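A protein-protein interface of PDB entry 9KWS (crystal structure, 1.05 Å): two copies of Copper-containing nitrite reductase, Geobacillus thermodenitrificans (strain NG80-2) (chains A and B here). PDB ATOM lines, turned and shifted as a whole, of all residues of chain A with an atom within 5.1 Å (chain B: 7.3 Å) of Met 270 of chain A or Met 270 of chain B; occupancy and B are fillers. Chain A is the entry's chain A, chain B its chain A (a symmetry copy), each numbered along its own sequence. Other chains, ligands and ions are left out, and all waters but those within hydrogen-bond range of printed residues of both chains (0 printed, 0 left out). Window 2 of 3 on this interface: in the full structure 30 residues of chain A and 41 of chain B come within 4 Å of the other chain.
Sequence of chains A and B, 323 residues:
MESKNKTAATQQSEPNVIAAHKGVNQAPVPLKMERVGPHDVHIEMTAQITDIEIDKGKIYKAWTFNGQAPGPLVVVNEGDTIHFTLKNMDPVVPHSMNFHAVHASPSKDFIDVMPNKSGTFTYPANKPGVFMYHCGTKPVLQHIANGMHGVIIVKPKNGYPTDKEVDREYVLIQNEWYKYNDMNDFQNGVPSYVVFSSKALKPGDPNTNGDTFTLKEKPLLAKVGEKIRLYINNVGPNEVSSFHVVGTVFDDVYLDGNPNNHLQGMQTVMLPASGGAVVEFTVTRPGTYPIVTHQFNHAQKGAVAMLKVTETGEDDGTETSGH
Among the printed residues, merely in contact across the chains: Val 240 of chain A with Val 240 of chain B, Ser 242 of chain A with Pro 272 of chain B, Thr 268 of chain A with Pro 272 of chain B, Thr 268 of chain A with Ala 273 of chain B, Met 270 of chain A with Val 240 of chain B, Met 270 of chain A with Met 270 of chain B, Met 270 of chain A with Pro 272 of chain B, Gln 295 of chain A with Val 240 of chain B and Gln 295 of chain A with Ala 273 of chain B.
The backbone NH (N) of Ala 273 of chain B lies within hydrogen-bond range of the side-chain hydroxyl (OG) of Ser 242 of chain A (3.0 Å).
Hydrophobic or aromatic side chains of chain B that line the printed part of chain A: Val 240, Met 270, Pro 272 and Ala 273.
Among the printed residues, 10 pairs touch across the chains.
The backbone carbonyl oxygen (O) of Val 240 of chain A sits at hydrogen-bond distance from the side-chain amide nitrogen (NE2) of Gln 295 of chain A (3.1 Å).
OG of Ser 242 of chain A lies within hydrogen-bond range of OE1 of Gln 295 of chain A.
The side-chain amide nitrogen of Asn 234 of chain B lies within hydrogen-bond range of the backbone carbonyl oxygen of Pro 272 of chain B, at 3.2 Å.
NE2 of Gln 295 of chain B lies within hydrogen-bond range of O of Val 240 of chain B (3.1 Å).
Ser 242 of chain A touches Pro 272 of chain B, but with the chains exchanged Pro 272 of chain A does not touch Ser 242 of chain B (12.2 Å).
Met 270 of chain A touches Val 240 of chain B, but with the chains exchanged Val 240 of chain A does not touch Met 270 of chain B (6.7 Å).
Met 270 of chain A touches Pro 272 of chain B, but with the chains exchanged Pro 272 of chain A does not touch Met 270 of chain B (7.9 Å).
Gln 295 of chain A touches Val 240 of chain B, but with the chains exchanged Val 240 of chain A does not touch Gln 295 of chain B (8.1 Å).
Of the 10 pairs that touch across the chains among the printed residues, 2 have their exchanged pair printed and touching as well.
Phe 243 of chain A touches none of the printed residues of chain B.
Printed residues of chain B within 4 Å of Met 270 of chain A: Val 240 (3.9 Å), Met 270 (3.97 Å) and Pro 272 (3.7 Å).
Asn 234 of chain B touches none of the printed residues of chain A.
Printed residues of chain A within 4 Å of Val 240 of chain B: Val 240, Met 270 and Gln 295.
Of the printed residues of chain A, Met 270 of chain B touches Met 270 (3.97 Å).
Printed residues of chain A within 4 Å of Ala 273 of chain B: Ser 242, Thr 268 and Gln 295.
The nearest printed residue of chain B that does not touch Met 270 of chain A is Leu 271 of chain B (4.3 Å).
The nearest printed residue of chain A that does not touch Met 270 of chain B is Val 240 of chain A (6.7 Å).
The nearest printed residue of chain A that does not touch Pro 272 of chain B is Val 269 of chain A (4.8 Å).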
ATOM      1  N   VAL A 240     -13.691 -29.958  -7.411  1.00  0.00           N
ATOM      2  CA  VAL A 240     -12.270 -30.257  -7.506  1.00  0.00           C
ATOM      3  C   VAL A 240     -11.485 -29.084  -6.924  1.00  0.00           C
ATOM      4  O   VAL A 240     -12.048 -28.011  -6.698  1.00  0.00           O
ATOM      5  CB  VAL A 240     -11.868 -30.599  -8.954  1.00  0.00           C
ATOM      6  CG1 VAL A 240     -12.703 -31.761  -9.462  1.00  0.00           C
ATOM      7  CG2 VAL A 240     -11.985 -29.407  -9.895  1.00  0.00           C
ATOM      8  N   SER A 241     -10.195 -29.287  -6.665  1.00  0.00           N
ATOM      9  CA  SER A 241      -9.361 -28.278  -6.025  1.00  0.00           C
ATOM     10  C   SER A 241      -8.083 -28.053  -6.814  1.00  0.00           C
ATOM     11  O   SER A 241      -7.462 -28.991  -7.307  1.00  0.00           O
ATOM     12  CB  SER A 241      -9.002 -28.701  -4.594  1.00  0.00           C
ATOM     13  OG  SER A 241      -8.107 -27.790  -3.994  1.00  0.00           O
ATOM     14  N   SER A 242      -7.677 -26.795  -6.895  1.00  0.00           N
ATOM     15  CA  SER A 242      -6.463 -26.367  -7.600  1.00  0.00           C
ATOM     16  C   SER A 242      -5.490 -25.858  -6.540  1.00  0.00           C
ATOM     17  O   SER A 242      -5.364 -24.663  -6.296  1.00  0.00           O
ATOM     18  CB  SER A 242      -6.832 -25.290  -8.619  1.00  0.00           C
ATOM     19  OG  SER A 242      -7.653 -25.819  -9.650  1.00  0.00           O
ATOM     20  N   PHE A 243      -4.808 -26.779  -5.854  1.00  0.00           N
ATOM     21  CA  PHE A 243      -4.139 -26.429  -4.608  1.00  0.00           C
ATOM     22  C   PHE A 243      -2.805 -25.721  -4.864  1.00  0.00           C
ATOM     23  O   PHE A 243      -1.965 -26.227  -5.609  1.00  0.00           O
ATOM     24  CB  PHE A 243      -3.916 -27.695  -3.781  1.00  0.00           C
ATOM     25  CG  PHE A 243      -3.370 -27.419  -2.427  1.00  0.00           C
ATOM     26  CD1 PHE A 243      -4.204 -27.034  -1.388  1.00  0.00           C
ATOM     27  CD2 PHE A 243      -2.000 -27.489  -2.189  1.00  0.00           C
ATOM     28  CE1 PHE A 243      -3.690 -26.760  -0.131  1.00  0.00           C
ATOM     29  CE2 PHE A 243      -1.490 -27.211  -0.933  1.00  0.00           C
ATOM     30  CZ  PHE A 243      -2.336 -26.854   0.094  1.00  0.00           C
ATOM     31  N   THR A 268       0.829 -25.844  -8.896  1.00  0.00           N
ATOM     32  CA  THR A 268      -0.536 -26.070  -8.448  1.00  0.00           C
ATOM     33  C   THR A 268      -0.846 -27.544  -8.653  1.00  0.00           C
ATOM     34  O   THR A 268      -0.483 -28.113  -9.688  1.00  0.00           O
ATOM     35  CB  THR A 268      -1.488 -25.175  -9.247  1.00  0.00           C
ATOM     36  OG1 THR A 268      -1.140 -23.830  -8.918  1.00  0.00           O
ATOM     37  CG2 THR A 268      -2.960 -25.448  -8.914  1.00  0.00           C
ATOM     38  N   VAL A 269      -1.511 -28.157  -7.681  1.00  0.00           N
ATOM     39  CA  VAL A 269      -1.839 -29.576  -7.735  1.00  0.00           C
ATOM     40  C   VAL A 269      -3.347 -29.740  -7.906  1.00  0.00           C
ATOM     41  O   VAL A 269      -4.127 -29.324  -7.047  1.00  0.00           O
ATOM     42  CB  VAL A 269      -1.341 -30.315  -6.484  1.00  0.00           C
ATOM     43  CG1 VAL A 269      -1.758 -31.777  -6.512  1.00  0.00           C
ATOM     44  CG2 VAL A 269       0.182 -30.201  -6.379  1.00  0.00           C
ATOM     45  N   MET A 270      -3.745 -30.376  -9.001  1.00  0.00           N
ATOM     46  CA  MET A 270      -5.143 -30.692  -9.294  1.00  0.00           C
ATOM     47  C   MET A 270      -5.583 -31.875  -8.437  1.00  0.00           C
ATOM     48  O   MET A 270      -5.017 -32.963  -8.559  1.00  0.00           O
ATOM     49  CB  MET A 270      -5.226 -31.082 -10.772  1.00  0.00           C
ATOM     50  CG  MET A 270      -6.579 -31.472 -11.309  1.00  0.00           C
ATOM     51  SD  MET A 270      -7.657 -30.135 -11.813  1.00  0.00           S
ATOM     52  CE  MET A 270      -8.343 -29.607 -10.238  1.00  0.00           C
ATOM     53  N   LEU A 271      -6.594 -31.676  -7.593  1.00  0.00           N
ATOM     54  CA  LEU A 271      -7.144 -32.744  -6.769  1.00  0.00           C
ATOM     55  C   LEU A 271      -8.576 -33.018  -7.182  1.00  0.00           C
ATOM     56  O   LEU A 271      -9.412 -32.102  -7.143  1.00  0.00           O
ATOM     57  CB  LEU A 271      -7.142 -32.371  -5.291  1.00  0.00           C
ATOM     58  CG  LEU A 271      -5.788 -32.063  -4.668  1.00  0.00           C
ATOM     59  CD1 LEU A 271      -5.975 -31.507  -3.280  1.00  0.00           C
ATOM     60  CD2 LEU A 271      -4.890 -33.285  -4.645  1.00  0.00           C
ATOM     61  N   PRO A 272      -8.922 -34.247  -7.544  1.00  0.00           N
ATOM     62  CA  PRO A 272     -10.338 -34.584  -7.731  1.00  0.00           C
ATOM     63  C   PRO A 272     -11.073 -34.476  -6.397  1.00  0.00           C
ATOM     64  O   PRO A 272     -10.464 -34.331  -5.334  1.00  0.00           O
ATOM     65  CB  PRO A 272     -10.293 -36.026  -8.247  1.00  0.00           C
ATOM     66  CG  PRO A 272      -9.014 -36.590  -7.679  1.00  0.00           C
ATOM     67  CD  PRO A 272      -8.048 -35.435  -7.649  1.00  0.00           C
ATOM     68  N   GLN A 295      -9.011 -21.969  -7.822  1.00  0.00           N
ATOM     69  CA  GLN A 295     -10.357 -21.678  -8.311  1.00  0.00           C
ATOM     70  C   GLN A 295     -10.855 -20.532  -7.439  1.00  0.00           C
ATOM     71  O   GLN A 295     -11.284 -20.745  -6.301  1.00  0.00           O
ATOM     72  CB  GLN A 295     -11.196 -22.938  -8.235  1.00  0.00           C
ATOM     73  CG  GLN A 295     -10.700 -23.984  -9.258  1.00  0.00           C
ATOM     74  CD  GLN A 295     -11.064 -25.404  -8.896  1.00  0.00           C
ATOM     75  OE1 GLN A 295     -10.196 -26.263  -8.776  1.00  0.00           O
ATOM     76  NE2 GLN A 295     -12.359 -25.670  -8.740  1.00  0.00           N
ATOM     77  N   ASN B 234      -3.840 -22.369 -18.081  1.00  0.00           N
ATOM     78  CA  ASN B 234      -5.218 -21.995 -17.813  1.00  0.00           C
ATOM     79  C   ASN B 234      -5.214 -21.071 -16.606  1.00  0.00           C
ATOM     80  O   ASN B 234      -5.074 -21.541 -15.475  1.00  0.00           O
ATOM     81  CB  ASN B 234      -6.024 -23.243 -17.485  1.00  0.00           C
ATOM     82  CG  ASN B 234      -7.356 -22.912 -16.906  1.00  0.00           C
ATOM     83  OD1 ASN B 234      -7.954 -21.885 -17.262  1.00  0.00           O
ATOM     84  ND2 ASN B 234      -7.849 -23.760 -16.015  1.00  0.00           N
ATOM     85  N   GLU B 239     -12.300 -21.811 -13.582  1.00  0.00           N
ATOM     86  CA  GLU B 239     -12.543 -23.102 -14.194  1.00  0.00           C
ATOM     87  C   GLU B 239     -11.254 -23.884 -14.355  1.00  0.00           C
ATOM     88  O   GLU B 239     -10.159 -23.321 -14.424  1.00  0.00           O
ATOM     89  CB  GLU B 239     -13.196 -22.940 -15.569  1.00  0.00           C
ATOM     90  CG  GLU B 239     -14.450 -22.107 -15.580  1.00  0.00           C
ATOM     91  CD  GLU B 239     -15.660 -22.726 -14.923  1.00  0.00           C
ATOM     92  OE1 GLU B 239     -15.699 -23.943 -14.681  1.00  0.00           O
ATOM     93  OE2 GLU B 239     -16.634 -21.981 -14.679  1.00  0.00           O
ATOM     94  N   VAL B 240     -11.405 -25.207 -14.418  1.00  0.00           N
ATOM     95  CA  VAL B 240     -10.357 -26.097 -14.893  1.00  0.00           C
ATOM     96  C   VAL B 240     -10.493 -26.245 -16.407  1.00  0.00           C
ATOM     97  O   VAL B 240     -11.514 -25.857 -16.979  1.00  0.00           O
ATOM     98  CB  VAL B 240     -10.388 -27.444 -14.145  1.00  0.00           C
ATOM     99  CG1 VAL B 240     -10.264 -27.209 -12.650  1.00  0.00           C
ATOM    100  CG2 VAL B 240     -11.636 -28.260 -14.454  1.00  0.00           C
ATOM    101  N   SER B 241      -9.466 -26.788 -17.057  1.00  0.00           N
ATOM    102  CA  SER B 241      -9.436 -26.901 -18.510  1.00  0.00           C
ATOM    103  C   SER B 241      -9.094 -28.318 -18.934  1.00  0.00           C
ATOM    104  O   SER B 241      -8.229 -28.968 -18.355  1.00  0.00           O
ATOM    105  CB  SER B 241      -8.406 -25.932 -19.106  1.00  0.00           C
ATOM    106  OG  SER B 241      -8.284 -26.101 -20.501  1.00  0.00           O
ATOM    107  N   SER B 242      -9.760 -28.774 -19.986  1.00  0.00           N
ATOM    108  CA  SER B 242      -9.569 -30.111 -20.562  1.00  0.00           C
ATOM    109  C   SER B 242      -8.951 -29.914 -21.944  1.00  0.00           C
ATOM    110  O   SER B 242      -9.629 -29.938 -22.966  1.00  0.00           O
ATOM    111  CB  SER B 242     -10.919 -30.825 -20.621  1.00  0.00           C
ATOM    112  OG  SER B 242     -11.419 -31.087 -19.319  1.00  0.00           O
ATOM    113  N   PHE B 243      -7.639 -29.669 -21.989  1.00  0.00           N
ATOM    114  CA  PHE B 243      -7.029 -29.125 -23.195  1.00  0.00           C
ATOM    115  C   PHE B 243      -6.803 -30.211 -24.251  1.00  0.00           C
ATOM    116  O   PHE B 243      -6.197 -31.244 -23.962  1.00  0.00           O
ATOM    117  CB  PHE B 243      -5.705 -28.453 -22.833  1.00  0.00           C
ATOM    118  CG  PHE B 243      -5.080 -27.741 -23.977  1.00  0.00           C
ATOM    119  CD1 PHE B 243      -5.490 -26.463 -24.330  1.00  0.00           C
ATOM    120  CD2 PHE B 243      -4.105 -28.365 -24.751  1.00  0.00           C
ATOM    121  CE1 PHE B 243      -4.918 -25.808 -25.409  1.00  0.00           C
ATOM    122  CE2 PHE B 243      -3.538 -27.708 -25.829  1.00  0.00           C
ATOM    123  CZ  PHE B 243      -3.941 -26.429 -26.152  1.00  0.00           C
ATOM    124  N   LEU B 255       3.990 -31.737 -17.322  1.00  0.00           N
ATOM    125  CA  LEU B 255       3.065 -31.002 -16.468  1.00  0.00           C
ATOM    126  C   LEU B 255       3.789 -29.831 -15.815  1.00  0.00           C
ATOM    127  O   LEU B 255       4.913 -29.975 -15.308  1.00  0.00           O
ATOM    128  CB  LEU B 255       2.449 -31.908 -15.408  1.00  0.00           C
ATOM    129  CG  LEU B 255       1.622 -33.072 -15.944  1.00  0.00           C
ATOM    130  CD1 LEU B 255       1.099 -33.876 -14.769  1.00  0.00           C
ATOM    131  CD2 LEU B 255       0.474 -32.601 -16.813  1.00  0.00           C
ATOM    132  N   MET B 266      -1.170 -38.570 -24.611  1.00  0.00           N
ATOM    133  CA  MET B 266      -2.405 -38.085 -24.002  1.00  0.00           C
ATOM    134  C   MET B 266      -3.319 -37.495 -25.067  1.00  0.00           C
ATOM    135  O   MET B 266      -2.872 -36.729 -25.921  1.00  0.00           O
ATOM    136  CB  MET B 266      -2.106 -37.009 -22.962  1.00  0.00           C
ATOM    137  CG  MET B 266      -1.226 -37.460 -21.801  1.00  0.00           C
ATOM    138  SD  MET B 266      -2.000 -38.611 -20.644  1.00  0.00           S
ATOM    139  CE  MET B 266      -3.292 -37.582 -19.947  1.00  0.00           C
ATOM    140  N   THR B 268      -5.931 -35.565 -24.045  1.00  0.00           N
ATOM    141  CA  THR B 268      -6.448 -34.366 -23.404  1.00  0.00           C
ATOM    142  C   THR B 268      -5.674 -34.169 -22.111  1.00  0.00           C
ATOM    143  O   THR B 268      -5.421 -35.137 -21.388  1.00  0.00           O
ATOM    144  CB  THR B 268      -7.949 -34.536 -23.146  1.00  0.00           C
ATOM    145  OG1 THR B 268      -8.564 -34.642 -24.429  1.00  0.00           O
ATOM    146  CG2 THR B 268      -8.539 -33.358 -22.360  1.00  0.00           C
ATOM    147  N   VAL B 269      -5.302 -32.928 -21.820  1.00  0.00           N
ATOM    148  CA  VAL B 269      -4.523 -32.606 -20.631  1.00  0.00           C
ATOM    149  C   VAL B 269      -5.393 -31.818 -19.656  1.00  0.00           C
ATOM    150  O   VAL B 269      -5.857 -30.720 -19.969  1.00  0.00           O
ATOM    151  CB  VAL B 269      -3.249 -31.826 -20.989  1.00  0.00           C
ATOM    152  CG1 VAL B 269      -2.486 -31.424 -19.737  1.00  0.00           C
ATOM    153  CG2 VAL B 269      -2.358 -32.668 -21.907  1.00  0.00           C
ATOM    154  N   MET B 270      -5.582 -32.372 -18.462  1.00  0.00           N
ATOM    155  CA  MET B 270      -6.321 -31.729 -17.377  1.00  0.00           C
ATOM    156  C   MET B 270      -5.450 -30.647 -16.746  1.00  0.00           C
ATOM    157  O   MET B 270      -4.381 -30.953 -16.215  1.00  0.00           O
ATOM    158  CB  MET B 270      -6.626 -32.805 -16.330  1.00  0.00           C
ATOM    159  CG  MET B 270      -7.374 -32.373 -15.095  1.00  0.00           C
ATOM    160  SD  MET B 270      -9.156 -32.284 -15.227  1.00  0.00           S
ATOM    161  CE  MET B 270      -9.385 -30.689 -16.021  1.00  0.00           C
ATOM    162  N   LEU B 271      -5.909 -29.396 -16.782  1.00  0.00           N
ATOM    163  CA  LEU B 271      -5.198 -28.288 -16.157  1.00  0.00           C
ATOM    164  C   LEU B 271      -6.032 -27.724 -15.024  1.00  0.00           C
ATOM    165  O   LEU B 271      -7.175 -27.302 -15.254  1.00  0.00           O
ATOM    166  CB  LEU B 271      -4.931 -27.162 -17.151  1.00  0.00           C
ATOM    167  CG  LEU B 271      -4.094 -27.516 -18.373  1.00  0.00           C
ATOM    168  CD1 LEU B 271      -4.104 -26.371 -19.352  1.00  0.00           C
ATOM    169  CD2 LEU B 271      -2.675 -27.891 -17.991  1.00  0.00           C
ATOM    170  N   PRO B 272      -5.507 -27.658 -13.806  1.00  0.00           N
ATOM    171  CA  PRO B 272      -6.205 -26.919 -12.749  1.00  0.00           C
ATOM    172  C   PRO B 272      -6.255 -25.435 -13.105  1.00  0.00           C
ATOM    173  O   PRO B 272      -5.602 -24.975 -14.045  1.00  0.00           O
ATOM    174  CB  PRO B 272      -5.347 -27.182 -11.507  1.00  0.00           C
ATOM    175  CG  PRO B 272      -3.963 -27.433 -12.052  1.00  0.00           C
ATOM    176  CD  PRO B 272      -4.173 -28.124 -13.373  1.00  0.00           C
ATOM    177  N   ALA B 273      -7.019 -24.669 -12.326  1.00  0.00           N
ATOM    178  CA  ALA B 273      -6.905 -23.219 -12.422  1.00  0.00           C
ATOM    179  C   ALA B 273      -5.496 -22.833 -11.993  1.00  0.00           C
ATOM    180  O   ALA B 273      -5.061 -23.239 -10.909  1.00  0.00           O
ATOM    181  CB  ALA B 273      -7.955 -22.550 -11.543  1.00  0.00           C
ATOM    182  N   GLY B 275      -2.992 -23.892 -13.796  1.00  0.00           N
ATOM    183  CA  GLY B 275      -2.150 -24.973 -14.243  1.00  0.00           C
ATOM    184  C   GLY B 275      -1.558 -24.745 -15.622  1.00  0.00           C
ATOM    185  O   GLY B 275      -2.203 -24.238 -16.540  1.00  0.00           O
ATOM    186  N   GLY B 276      -0.311 -25.185 -15.765  1.00  0.00           N
ATOM    187  CA  GLY B 276       0.411 -25.079 -17.011  1.00  0.00           C
ATOM    188  C   GLY B 276       0.866 -26.432 -17.540  1.00  0.00           C
ATOM    189  O   GLY B 276       0.813 -27.460 -16.851  1.00  0.00           O
ATOM    190  N   ALA B 277       1.352 -26.410 -18.775  1.00  0.00           N
ATOM    191  CA  ALA B 277       1.951 -27.589 -19.372  1.00  0.00           C
ATOM    192  C   ALA B 277       2.752 -27.168 -20.592  1.00  0.00           C
ATOM    193  O   ALA B 277       2.520 -26.112 -21.184  1.00  0.00           O
ATOM    194  CB  ALA B 277       0.916 -28.635 -19.795  1.00  0.00           C
ATOM    195  N   THR B 293     -10.796 -26.319 -25.166  1.00  0.00           N
ATOM    196  CA  THR B 293     -11.085 -27.025 -23.929  1.00  0.00           C
ATOM    197  C   THR B 293     -12.269 -27.946 -24.220  1.00  0.00           C
ATOM    198  O   THR B 293     -13.273 -27.520 -24.805  1.00  0.00           O
ATOM    199  CB  THR B 293     -11.351 -26.121 -22.727  1.00  0.00           C
ATOM    200  OG1 THR B 293     -11.705 -26.990 -21.642  1.00  0.00           O
ATOM    201  CG2 THR B 293     -12.454 -25.111 -22.980  1.00  0.00           C
ATOM    202  N   GLN B 295     -14.308 -29.282 -22.217  1.00  0.00           N
ATOM    203  CA  GLN B 295     -15.514 -28.898 -21.486  1.00  0.00           C
ATOM    204  C   GLN B 295     -16.313 -28.044 -22.463  1.00  0.00           C
ATOM    205  O   GLN B 295     -16.019 -26.862 -22.656  1.00  0.00           O
ATOM    206  CB  GLN B 295     -15.113 -28.185 -20.209  1.00  0.00           C
ATOM    207  CG  GLN B 295     -14.439 -29.169 -19.227  1.00  0.00           C
ATOM    208  CD  GLN B 295     -13.533 -28.496 -18.224  1.00  0.00           C
ATOM    209  OE1 GLN B 295     -12.352 -28.818 -18.129  1.00  0.00           O
ATOM    210  NE2 GLN B 295     -14.084 -27.566 -17.448  1.00  0.00           N
